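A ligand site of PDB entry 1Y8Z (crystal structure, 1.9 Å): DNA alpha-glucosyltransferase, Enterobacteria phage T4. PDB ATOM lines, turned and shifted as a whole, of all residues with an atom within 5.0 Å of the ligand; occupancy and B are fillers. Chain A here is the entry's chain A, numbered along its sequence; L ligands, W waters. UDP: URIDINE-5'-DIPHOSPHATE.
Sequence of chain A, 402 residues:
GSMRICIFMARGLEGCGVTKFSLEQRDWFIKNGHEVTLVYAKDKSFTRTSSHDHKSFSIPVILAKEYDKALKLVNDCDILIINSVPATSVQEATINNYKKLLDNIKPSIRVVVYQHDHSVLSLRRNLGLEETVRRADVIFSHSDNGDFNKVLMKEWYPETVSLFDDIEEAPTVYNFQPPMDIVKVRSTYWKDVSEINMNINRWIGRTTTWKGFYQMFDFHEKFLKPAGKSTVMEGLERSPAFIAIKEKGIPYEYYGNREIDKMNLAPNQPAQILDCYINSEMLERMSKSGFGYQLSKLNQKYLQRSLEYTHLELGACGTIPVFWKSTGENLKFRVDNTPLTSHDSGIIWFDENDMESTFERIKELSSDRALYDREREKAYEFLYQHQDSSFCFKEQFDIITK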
ATOM      1  N   GLY A  15      -3.763 -15.317  34.685  1.00  0.00           N
ATOM      2  CA  GLY A  15      -4.965 -15.105  33.897  1.00  0.00           C
ATOM      3  C   GLY A  15      -4.892 -14.144  32.735  1.00  0.00           C
ATOM      4  O   GLY A  15      -5.910 -13.850  32.107  1.00  0.00           O
ATOM      5  N   CME A  16      -3.696 -13.653  32.440  1.00  0.00           N
ATOM      6  CA  CME A  16      -3.531 -12.727  31.323  1.00  0.00           C
ATOM      7  CB  CME A  16      -2.901 -11.430  31.825  1.00  0.00           C
ATOM      8  SG  CME A  16      -4.117 -10.426  32.745  1.00  0.00           S
ATOM      9  SD  CME A  16      -3.867 -10.934  34.696  1.00  0.00           S
ATOM     10  CE  CME A  16      -2.288 -10.158  35.177  1.00  0.00           C
ATOM     11  CZ  CME A  16      -2.125  -8.796  34.566  1.00  0.00           C
ATOM     12  OH  CME A  16      -1.428  -8.790  33.503  1.00  0.00           O
ATOM     13  C   CME A  16      -2.736 -13.337  30.163  1.00  0.00           C
ATOM     14  O   CME A  16      -2.947 -14.489  29.831  1.00  0.00           O
ATOM     15  N   GLY A  17      -1.832 -12.567  29.563  1.00  0.00           N
ATOM     16  CA  GLY A  17      -1.061 -13.055  28.429  1.00  0.00           C
ATOM     17  C   GLY A  17      -0.130 -14.238  28.647  1.00  0.00           C
ATOM     18  O   GLY A  17       0.073 -15.066  27.734  1.00  0.00           O
ATOM     19  N   VAL A  18       0.457 -14.328  29.835  1.00  0.00           N
ATOM     20  CA  VAL A  18       1.363 -15.431  30.118  1.00  0.00           C
ATOM     21  C   VAL A  18       0.558 -16.716  30.267  1.00  0.00           C
ATOM     22  O   VAL A  18       0.949 -17.762  29.772  1.00  0.00           O
ATOM     23  CB  VAL A  18       2.211 -15.136  31.382  1.00  0.00           C
ATOM     24  CG1 VAL A  18       3.225 -16.266  31.625  1.00  0.00           C
ATOM     25  CG2 VAL A  18       2.945 -13.806  31.209  1.00  0.00           C
ATOM     26  N   LYS A  20      -2.456 -17.229  28.957  1.00  0.00           N
ATOM     27  CA  LYS A  20      -2.976 -17.529  27.625  1.00  0.00           C
ATOM     28  C   LYS A  20      -1.915 -18.196  26.755  1.00  0.00           C
ATOM     29  O   LYS A  20      -2.202 -19.177  26.074  1.00  0.00           O
ATOM     30  CB  LYS A  20      -3.474 -16.240  26.945  1.00  0.00           C
ATOM     31  CG  LYS A  20      -3.971 -16.425  25.515  1.00  0.00           C
ATOM     32  CD  LYS A  20      -5.136 -17.392  25.445  1.00  0.00           C
ATOM     33  CE  LYS A  20      -5.736 -17.444  24.038  1.00  0.00           C
ATOM     34  NZ  LYS A  20      -6.829 -18.462  23.978  1.00  0.00           N
ATOM     35  N   ARG A  48      -7.874 -12.862  38.021  1.00  0.00           N
ATOM     36  CA  ARG A  48      -8.306 -13.490  36.774  1.00  0.00           C
ATOM     37  C   ARG A  48      -7.994 -14.975  36.591  1.00  0.00           C
ATOM     38  O   ARG A  48      -7.907 -15.463  35.465  1.00  0.00           O
ATOM     39  CB  ARG A  48      -7.737 -12.710  35.575  1.00  0.00           C
ATOM     40  CG  ARG A  48      -7.956 -11.198  35.626  1.00  0.00           C
ATOM     41  CD  ARG A  48      -7.275 -10.509  34.435  1.00  0.00           C
ATOM     42  NE  ARG A  48      -6.949  -9.104  34.684  1.00  0.00           N
ATOM     43  CZ  ARG A  48      -7.791  -8.087  34.494  1.00  0.00           C
ATOM     44  NH1 ARG A  48      -9.018  -8.290  34.053  1.00  0.00           N
ATOM     45  NH2 ARG A  48      -7.384  -6.839  34.752  1.00  0.00           N
ATOM     46  N   SER A  51     -10.477 -16.563  34.298  1.00  0.00           N
ATOM     47  CA  SER A  51     -10.704 -16.004  32.963  1.00  0.00           C
ATOM     48  C   SER A  51     -10.513 -17.036  31.856  1.00  0.00           C
ATOM     49  O   SER A  51     -11.261 -17.052  30.879  1.00  0.00           O
ATOM     50  CB  SER A  51      -9.773 -14.802  32.736  1.00  0.00           C
ATOM     51  OG  SER A  51      -8.415 -15.217  32.732  1.00  0.00           O
ATOM     52  N   HIS A  52      -9.503 -17.888  32.003  1.00  0.00           N
ATOM     53  CA  HIS A  52      -9.219 -18.928  31.014  1.00  0.00           C
ATOM     54  C   HIS A  52      -9.603 -20.312  31.553  1.00  0.00           C
ATOM     55  O   HIS A  52      -9.533 -20.553  32.755  1.00  0.00           O
ATOM     56  CB  HIS A  52      -7.739 -18.914  30.629  1.00  0.00           C
ATOM     57  CG  HIS A  52      -7.294 -17.634  29.999  1.00  0.00           C
ATOM     58  ND1 HIS A  52      -6.723 -16.603  30.716  1.00  0.00           N
ATOM     59  CD2 HIS A  52      -7.372 -17.201  28.720  1.00  0.00           C
ATOM     60  CE1 HIS A  52      -6.461 -15.599  29.898  1.00  0.00           C
ATOM     61  NE2 HIS A  52      -6.853 -15.936  28.683  1.00  0.00           N
ATOM     62  N   GLY A 205      -8.761  -4.747  27.275  1.00  0.00           N
ATOM     63  CA  GLY A 205      -7.431  -4.455  27.736  1.00  0.00           C
ATOM     64  C   GLY A 205      -7.291  -4.632  29.232  1.00  0.00           C
ATOM     65  O   GLY A 205      -7.926  -5.503  29.811  1.00  0.00           O
ATOM     66  N   ARG A 206      -6.449  -3.804  29.833  1.00  0.00           N
ATOM     67  CA  ARG A 206      -6.191  -3.834  31.273  1.00  0.00           C
ATOM     68  C   ARG A 206      -5.992  -2.410  31.740  1.00  0.00           C
ATOM     69  O   ARG A 206      -5.825  -1.503  30.920  1.00  0.00           O
ATOM     70  CB  ARG A 206      -4.894  -4.594  31.576  1.00  0.00           C
ATOM     71  CG  ARG A 206      -5.008  -6.072  31.696  1.00  0.00           C
ATOM     72  CD  ARG A 206      -3.763  -6.610  32.365  1.00  0.00           C
ATOM     73  NE  ARG A 206      -2.577  -6.602  31.514  1.00  0.00           N
ATOM     74  CZ  ARG A 206      -1.480  -5.884  31.731  1.00  0.00           C
ATOM     75  NH1 ARG A 206      -0.451  -5.962  30.899  1.00  0.00           N
ATOM     76  NH2 ARG A 206      -1.408  -5.076  32.790  1.00  0.00           N
ATOM     77  N   TRP A 210      -0.405   2.017  28.874  1.00  0.00           N
ATOM     78  CA  TRP A 210      -0.071   1.677  27.496  1.00  0.00           C
ATOM     79  C   TRP A 210      -1.115   0.846  26.771  1.00  0.00           C
ATOM     80  O   TRP A 210      -0.905   0.483  25.598  1.00  0.00           O
ATOM     81  CB  TRP A 210       1.302   1.006  27.405  1.00  0.00           C
ATOM     82  CG  TRP A 210       1.501  -0.249  28.205  1.00  0.00           C
ATOM     83  CD1 TRP A 210       1.956  -0.335  29.501  1.00  0.00           C
ATOM     84  CD2 TRP A 210       1.335  -1.592  27.747  1.00  0.00           C
ATOM     85  NE1 TRP A 210       2.102  -1.657  29.858  1.00  0.00           N
ATOM     86  CE2 TRP A 210       1.723  -2.447  28.801  1.00  0.00           C
ATOM     87  CE3 TRP A 210       0.893  -2.155  26.542  1.00  0.00           C
ATOM     88  CZ2 TRP A 210       1.691  -3.836  28.695  1.00  0.00           C
ATOM     89  CZ3 TRP A 210       0.872  -3.541  26.427  1.00  0.00           C
ATOM     90  CH2 TRP A 210       1.265  -4.368  27.501  1.00  0.00           C
ATOM     91  N   LYS A 211      -2.224   0.522  27.443  1.00  0.00           N
ATOM     92  CA  LYS A 211      -3.303  -0.236  26.815  1.00  0.00           C
ATOM     93  C   LYS A 211      -4.276   0.764  26.163  1.00  0.00           C
ATOM     94  O   LYS A 211      -5.273   0.368  25.559  1.00  0.00           O
ATOM     95  CB  LYS A 211      -4.052  -1.089  27.851  1.00  0.00           C
ATOM     96  CG  LYS A 211      -3.225  -2.248  28.394  1.00  0.00           C
ATOM     97  CD  LYS A 211      -3.022  -3.347  27.368  1.00  0.00           C
ATOM     98  CE  LYS A 211      -2.281  -4.540  28.001  1.00  0.00           C
ATOM     99  NZ  LYS A 211      -2.095  -5.661  27.051  1.00  0.00           N
ATOM    100  N   GLY A 235     -12.202  -5.490  30.906  1.00  0.00           N
ATOM    101  CA  GLY A 235     -10.901  -5.751  31.485  1.00  0.00           C
ATOM    102  C   GLY A 235     -10.286  -4.646  32.329  1.00  0.00           C
ATOM    103  O   GLY A 235      -9.208  -4.850  32.897  1.00  0.00           O
ATOM    104  N   ASP A 275     -15.160  -5.102  34.755  1.00  0.00           N
ATOM    105  CA  ASP A 275     -14.014  -5.398  35.625  1.00  0.00           C
ATOM    106  C   ASP A 275     -12.997  -6.401  35.076  1.00  0.00           C
ATOM    107  O   ASP A 275     -11.819  -6.075  34.876  1.00  0.00           O
ATOM    108  CB  ASP A 275     -14.556  -5.898  36.967  1.00  0.00           C
ATOM    109  CG  ASP A 275     -13.485  -6.076  38.011  1.00  0.00           C
ATOM    110  OD1 ASP A 275     -13.844  -6.337  39.183  1.00  0.00           O
ATOM    111  OD2 ASP A 275     -12.296  -5.941  37.675  1.00  0.00           O
ATOM    112  N   CME A 276     -13.431  -7.635  34.887  1.00  0.00           N
ATOM    113  CA  CME A 276     -12.594  -8.683  34.348  1.00  0.00           C
ATOM    114  CB  CME A 276     -11.827  -9.407  35.453  1.00  0.00           C
ATOM    115  SG  CME A 276     -12.849 -10.379  36.596  1.00  0.00           S
ATOM    116  SD  CME A 276     -11.983 -12.222  36.529  1.00  0.00           S
ATOM    117  CE  CME A 276     -12.886 -13.071  35.190  1.00  0.00           C
ATOM    118  CZ  CME A 276     -14.375 -12.863  35.287  1.00  0.00           C
ATOM    119  OH  CME A 276     -14.882 -13.228  36.410  1.00  0.00           O
ATOM    120  C   CME A 276     -13.564  -9.617  33.648  1.00  0.00           C
ATOM    121  O   CME A 276     -14.733  -9.712  34.055  1.00  0.00           O
ATOM    122  N   TYR A 277     -13.111 -10.308  32.619  1.00  0.00           N
ATOM    123  CA  TYR A 277     -14.010 -11.174  31.876  1.00  0.00           C
ATOM    124  C   TYR A 277     -13.534 -12.600  31.669  1.00  0.00           C
ATOM    125  O   TYR A 277     -12.348 -12.915  31.801  1.00  0.00           O
ATOM    126  CB  TYR A 277     -14.295 -10.530  30.517  1.00  0.00           C
ATOM    127  CG  TYR A 277     -13.043 -10.258  29.681  1.00  0.00           C
ATOM    128  CD1 TYR A 277     -12.530 -11.232  28.831  1.00  0.00           C
ATOM    129  CD2 TYR A 277     -12.390  -9.026  29.745  1.00  0.00           C
ATOM    130  CE1 TYR A 277     -11.399 -10.999  28.061  1.00  0.00           C
ATOM    131  CE2 TYR A 277     -11.252  -8.775  28.968  1.00  0.00           C
ATOM    132  CZ  TYR A 277     -10.764  -9.765  28.138  1.00  0.00           C
ATOM    133  OH  TYR A 277      -9.637  -9.541  27.371  1.00  0.00           O
ATOM    134  N   ILE A 278     -14.493 -13.469  31.356  1.00  0.00           N
ATOM    135  CA  ILE A 278     -14.216 -14.865  31.058  1.00  0.00           C
ATOM    136  C   ILE A 278     -13.920 -14.795  29.567  1.00  0.00           C
ATOM    137  O   ILE A 278     -14.740 -14.320  28.786  1.00  0.00           O
ATOM    138  CB  ILE A 278     -15.457 -15.753  31.277  1.00  0.00           C
ATOM    139  CG1 ILE A 278     -15.893 -15.693  32.742  1.00  0.00           C
ATOM    140  CG2 ILE A 278     -15.158 -17.172  30.815  1.00  0.00           C
ATOM    141  CD1 ILE A 278     -14.882 -16.231  33.734  1.00  0.00           C
ATOM    142  N   ASN A 279     -12.731 -15.263  29.180  1.00  0.00           N
ATOM    143  CA  ASN A 279     -12.304 -15.189  27.792  1.00  0.00           C
ATOM    144  C   ASN A 279     -13.358 -15.628  26.772  1.00  0.00           C
ATOM    145  O   ASN A 279     -13.678 -14.876  25.834  1.00  0.00           O
ATOM    146  CB  ASN A 279     -11.015 -16.002  27.619  1.00  0.00           C
ATOM    147  CG  ASN A 279     -10.333 -15.755  26.284  1.00  0.00           C
ATOM    148  OD1 ASN A 279     -10.438 -16.569  25.361  1.00  0.00           O
ATOM    149  ND2 ASN A 279      -9.632 -14.627  26.180  1.00  0.00           N
ATOM    150  N   MET A 282     -16.223 -13.148  26.438  1.00  0.00           N
ATOM    151  CA  MET A 282     -15.844 -11.920  25.747  1.00  0.00           C
ATOM    152  C   MET A 282     -15.787 -12.156  24.234  1.00  0.00           C
ATOM    153  O   MET A 282     -16.226 -11.302  23.466  1.00  0.00           O
ATOM    154  CB  MET A 282     -14.469 -11.448  26.254  1.00  0.00           C
ATOM    155  CG  MET A 282     -13.894 -10.193  25.554  1.00  0.00           C
ATOM    156  SD  MET A 282     -13.192 -10.492  23.903  1.00  0.00           S
ATOM    157  CE  MET A 282     -11.574 -11.198  24.329  1.00  0.00           C
ATOM    158  N   GLN A 294      -8.125  -2.334  20.361  1.00  0.00           N
ATOM    159  CA  GLN A 294      -6.969  -2.816  21.107  1.00  0.00           C
ATOM    160  C   GLN A 294      -6.011  -1.673  20.875  1.00  0.00           C
ATOM    161  O   GLN A 294      -5.365  -1.585  19.822  1.00  0.00           O
ATOM    162  CB  GLN A 294      -6.441  -4.131  20.509  1.00  0.00           C
ATOM    163  CG  GLN A 294      -5.782  -5.049  21.552  1.00  0.00           C
ATOM    164  CD  GLN A 294      -4.432  -4.550  22.040  1.00  0.00           C
ATOM    165  OE1 GLN A 294      -4.005  -3.451  21.717  1.00  0.00           O
ATOM    166  NE2 GLN A 294      -3.745  -5.375  22.834  1.00  0.00           N
ATOM    167  N   GLU A 308      -0.440  -8.693  20.601  1.00  0.00           N
ATOM    168  CA  GLU A 308      -0.847  -9.330  21.849  1.00  0.00           C
ATOM    169  C   GLU A 308      -2.056 -10.200  21.583  1.00  0.00           C
ATOM    170  O   GLU A 308      -2.696 -10.079  20.546  1.00  0.00           O
ATOM    171  CB  GLU A 308      -1.186  -8.259  22.889  1.00  0.00           C
ATOM    172  CG  GLU A 308       0.006  -7.367  23.229  1.00  0.00           C
ATOM    173  CD  GLU A 308      -0.345  -6.277  24.215  1.00  0.00           C
ATOM    174  OE1 GLU A 308      -1.104  -5.360  23.843  1.00  0.00           O
ATOM    175  OE2 GLU A 308       0.135  -6.344  25.369  1.00  0.00           O
ATOM    176  N   TYR A 309      -2.361 -11.098  22.516  1.00  0.00           N
ATOM    177  CA  TYR A 309      -3.508 -11.973  22.342  1.00  0.00           C
ATOM    178  C   TYR A 309      -4.800 -11.206  22.097  1.00  0.00           C
ATOM    179  O   TYR A 309      -5.626 -11.625  21.281  1.00  0.00           O
ATOM    180  CB  TYR A 309      -3.666 -12.899  23.567  1.00  0.00           C
ATOM    181  CG  TYR A 309      -2.697 -14.054  23.495  1.00  0.00           C
ATOM    182  CD1 TYR A 309      -1.595 -14.122  24.338  1.00  0.00           C
ATOM    183  CD2 TYR A 309      -2.840 -15.023  22.508  1.00  0.00           C
ATOM    184  CE1 TYR A 309      -0.654 -15.142  24.194  1.00  0.00           C
ATOM    185  CE2 TYR A 309      -1.901 -16.034  22.353  1.00  0.00           C
ATOM    186  CZ  TYR A 309      -0.810 -16.089  23.190  1.00  0.00           C
ATOM    187  OH  TYR A 309       0.136 -17.059  22.966  1.00  0.00           O
ATOM    188  N   THR A 310      -4.985 -10.074  22.760  1.00  0.00           N
ATOM    189  CA  THR A 310      -6.207  -9.301  22.549  1.00  0.00           C
ATOM    190  C   THR A 310      -6.275  -8.769  21.110  1.00  0.00           C
ATOM    191  O   THR A 310      -7.362  -8.577  20.562  1.00  0.00           O
ATOM    192  CB  THR A 310      -6.350  -8.159  23.579  1.00  0.00           C
ATOM    193  OG1 THR A 310      -5.125  -7.431  23.689  1.00  0.00           O
ATOM    194  CG2 THR A 310      -6.722  -8.745  24.947  1.00  0.00           C
ATOM    195  N   GLU A 313      -7.383 -11.864  19.081  1.00  0.00           N
ATOM    196  CA  GLU A 313      -8.751 -12.238  19.398  1.00  0.00           C
ATOM    197  C   GLU A 313      -9.789 -11.437  18.627  1.00  0.00           C
ATOM    198  O   GLU A 313     -10.838 -11.969  18.279  1.00  0.00           O
ATOM    199  CB  GLU A 313      -8.989 -12.107  20.912  1.00  0.00           C
ATOM    200  CG  GLU A 313      -8.385 -13.272  21.682  1.00  0.00           C
ATOM    201  CD  GLU A 313      -8.241 -13.028  23.171  1.00  0.00           C
ATOM    202  OE1 GLU A 313      -7.990 -14.016  23.884  1.00  0.00           O
ATOM    203  OE2 GLU A 313      -8.370 -11.868  23.630  1.00  0.00           O
HETATM  204  N1  UDP L   1      -8.155 -11.803  29.366  1.00  0.00           N
HETATM  205  C2  UDP L   1      -9.290 -12.412  29.881  1.00  0.00           C
HETATM  206  N3  UDP L   1      -9.912 -11.715  30.884  1.00  0.00           N
HETATM  207  C4  UDP L   1      -9.530 -10.497  31.411  1.00  0.00           C
HETATM  208  C5  UDP L   1      -8.342  -9.938  30.821  1.00  0.00           C
HETATM  209  C6  UDP L   1      -7.713 -10.593  29.848  1.00  0.00           C
HETATM  210  O2  UDP L   1      -9.721 -13.475  29.471  1.00  0.00           O
HETATM  211  O4  UDP L   1     -10.171 -10.014  32.338  1.00  0.00           O
HETATM  212  C1' UDP L   1      -7.417 -12.492  28.301  1.00  0.00           C
HETATM  213  C2' UDP L   1      -7.382 -11.745  26.976  1.00  0.00           C
HETATM  214  O2' UDP L   1      -8.563 -12.022  26.255  1.00  0.00           O
HETATM  215  C3' UDP L   1      -6.117 -12.339  26.363  1.00  0.00           C
HETATM  216  C4' UDP L   1      -5.184 -12.434  27.569  1.00  0.00           C
HETATM  217  O4' UDP L   1      -6.068 -12.593  28.714  1.00  0.00           O
HETATM  218  O3' UDP L   1      -6.402 -13.653  25.906  1.00  0.00           O
HETATM  219  C5' UDP L   1      -4.261 -11.252  27.784  1.00  0.00           C
HETATM  220  O5' UDP L   1      -3.172 -11.287  26.857  1.00  0.00           O
HETATM  221  PA  UDP L   1      -2.579  -9.959  26.190  1.00  0.00           P
HETATM  222  O1A UDP L   1      -1.193 -10.266  25.787  1.00  0.00           O
HETATM  223  O2A UDP L   1      -3.559  -9.498  25.179  1.00  0.00           O
HETATM  224  O3A UDP L   1      -2.610  -8.832  27.373  1.00  0.00           O
HETATM  225  PB  UDP L   1      -1.808  -8.725  28.792  1.00  0.00           P
HETATM  226  O1B UDP L   1      -0.745  -7.692  28.637  1.00  0.00           O
HETATM  227  O2B UDP L   1      -2.859  -8.531  29.797  1.00  0.00           O
HETATM  228  O3B UDP L   1      -1.102 -10.130  28.987  1.00  0.00           O
HETATM  229  O   HOH W   1      -4.514  -6.440  26.320  1.00  0.00           O
HETATM  230  O   HOH W   2       0.569 -10.666  31.320  1.00  0.00           O
HETATM  231  O   HOH W   3      -7.669  -7.751  28.331  1.00  0.00           O
HETATM  232  O   HOH W   4       2.148 -10.462  28.676  1.00  0.00           O
HETATM  233  O   HOH W   5       2.723  -7.761  28.776  1.00  0.00           O
HETATM  234  O   HOH W   6      -5.295  -7.407  28.628  1.00  0.00           O
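Water W6 lies within hydrogen-bond range of an oxygen (O2B) of the ligand (2.9 Å) and the backbone carbonyl oxygen (O) of Gly 205 (3.5 Å).
Water W3 bridges the backbone carbonyl oxygen of Gly 205 and the side-chain hydroxyl of Tyr 277.
Water W1 lies within hydrogen-bond range of the side-chain amino group of Lys 211 (2.6 Å), the side-chain hydroxyl of Thr 310 (2.9 Å) and an oxygen (O3A) of the ligand (3.2 Å).
The side-chain carboxylate of Glu 313 sits at hydrogen-bond distance from the side-chain amide nitrogen of Asn 279.
OH of CME 16 is in hydrogen-bond range of NE of Arg 206, 3.2 Å away.
NE of Arg 48 sits close to SD of CME 16 (3.6 Å).
The backbone carbonyl oxygen of Arg 48 lies within hydrogen-bond range of the side-chain hydroxyl of Ser 51.
OG1 of Thr 310 lies within hydrogen-bond range of NE2 of Gln 294, at 2.6 Å.
The side-chain amino group (NZ) of Lys 211 is in salt-bridge range of the side-chain carboxylate (OE2) of Glu 308.
A ring nitrogen (ND1) of His 52 lies close to the backbone carbonyl oxygen (O) of Gly 15, 3.2 Å away.
O of Gly 15 sits at hydrogen-bond distance from OG of Ser 51 (2.9 Å).
An oxygen (O2B) of the ligand sits close to SG of CME 16 (3.7 Å).
Residues that only touch the ligand: Gly 15, Lys 20, Ser 51, CME 276, Met 282 and Glu 308.
Of the 24 residues printed, 17 come within 4 Å of the ligand.
Along chain A the residues within 4 Å of the ligand span positions 15 to 313.
The nearest printed residue that does not touch the ligand is Trp 210 (4.05 Å).
An oxygen (O3') of the ligand lies within hydrogen-bond range of the side-chain carboxylate (OE1) of Glu 313.
NE of Arg 206 lies within salt-bridge range of O2B of the ligand.
O3B of the ligand is in hydrogen-bond range of N of Gly 17 (2.6 Å).
NH1 of Arg 48 is in hydrogen-bond range of O4 of the ligand, 2.7 Å away.
The side-chain amide nitrogen of Asn 279 is in hydrogen-bond range of an oxygen (O2') of the ligand (2.8 Å).
O2A of the ligand sits at hydrogen-bond distance from N of Thr 310 (2.9 Å).
The side-chain hydroxyl (OG1) of Thr 310 lies within hydrogen-bond range of an oxygen (O2A) of the ligand, 3.0 Å away.
O4 of the ligand is in hydrogen-bond range of N of Tyr 277, 3.0 Å away.
The backbone carbonyl oxygen (O) of Tyr 277 is in hydrogen-bond range of a nitrogen (N3) of the ligand (2.9 Å).
O2' of the ligand lies within hydrogen-bond range of OH of Tyr 277 (2.9 Å).
The side-chain amino group of Lys 211 lies within salt-bridge range of an oxygen (O1B) of the ligand, 2.9 Å away.
NE2 of His 52 sits close to O4' of the ligand.
The backbone NH of Tyr 309 sits at hydrogen-bond distance from an oxygen (O2A) of the ligand (3.3 Å).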
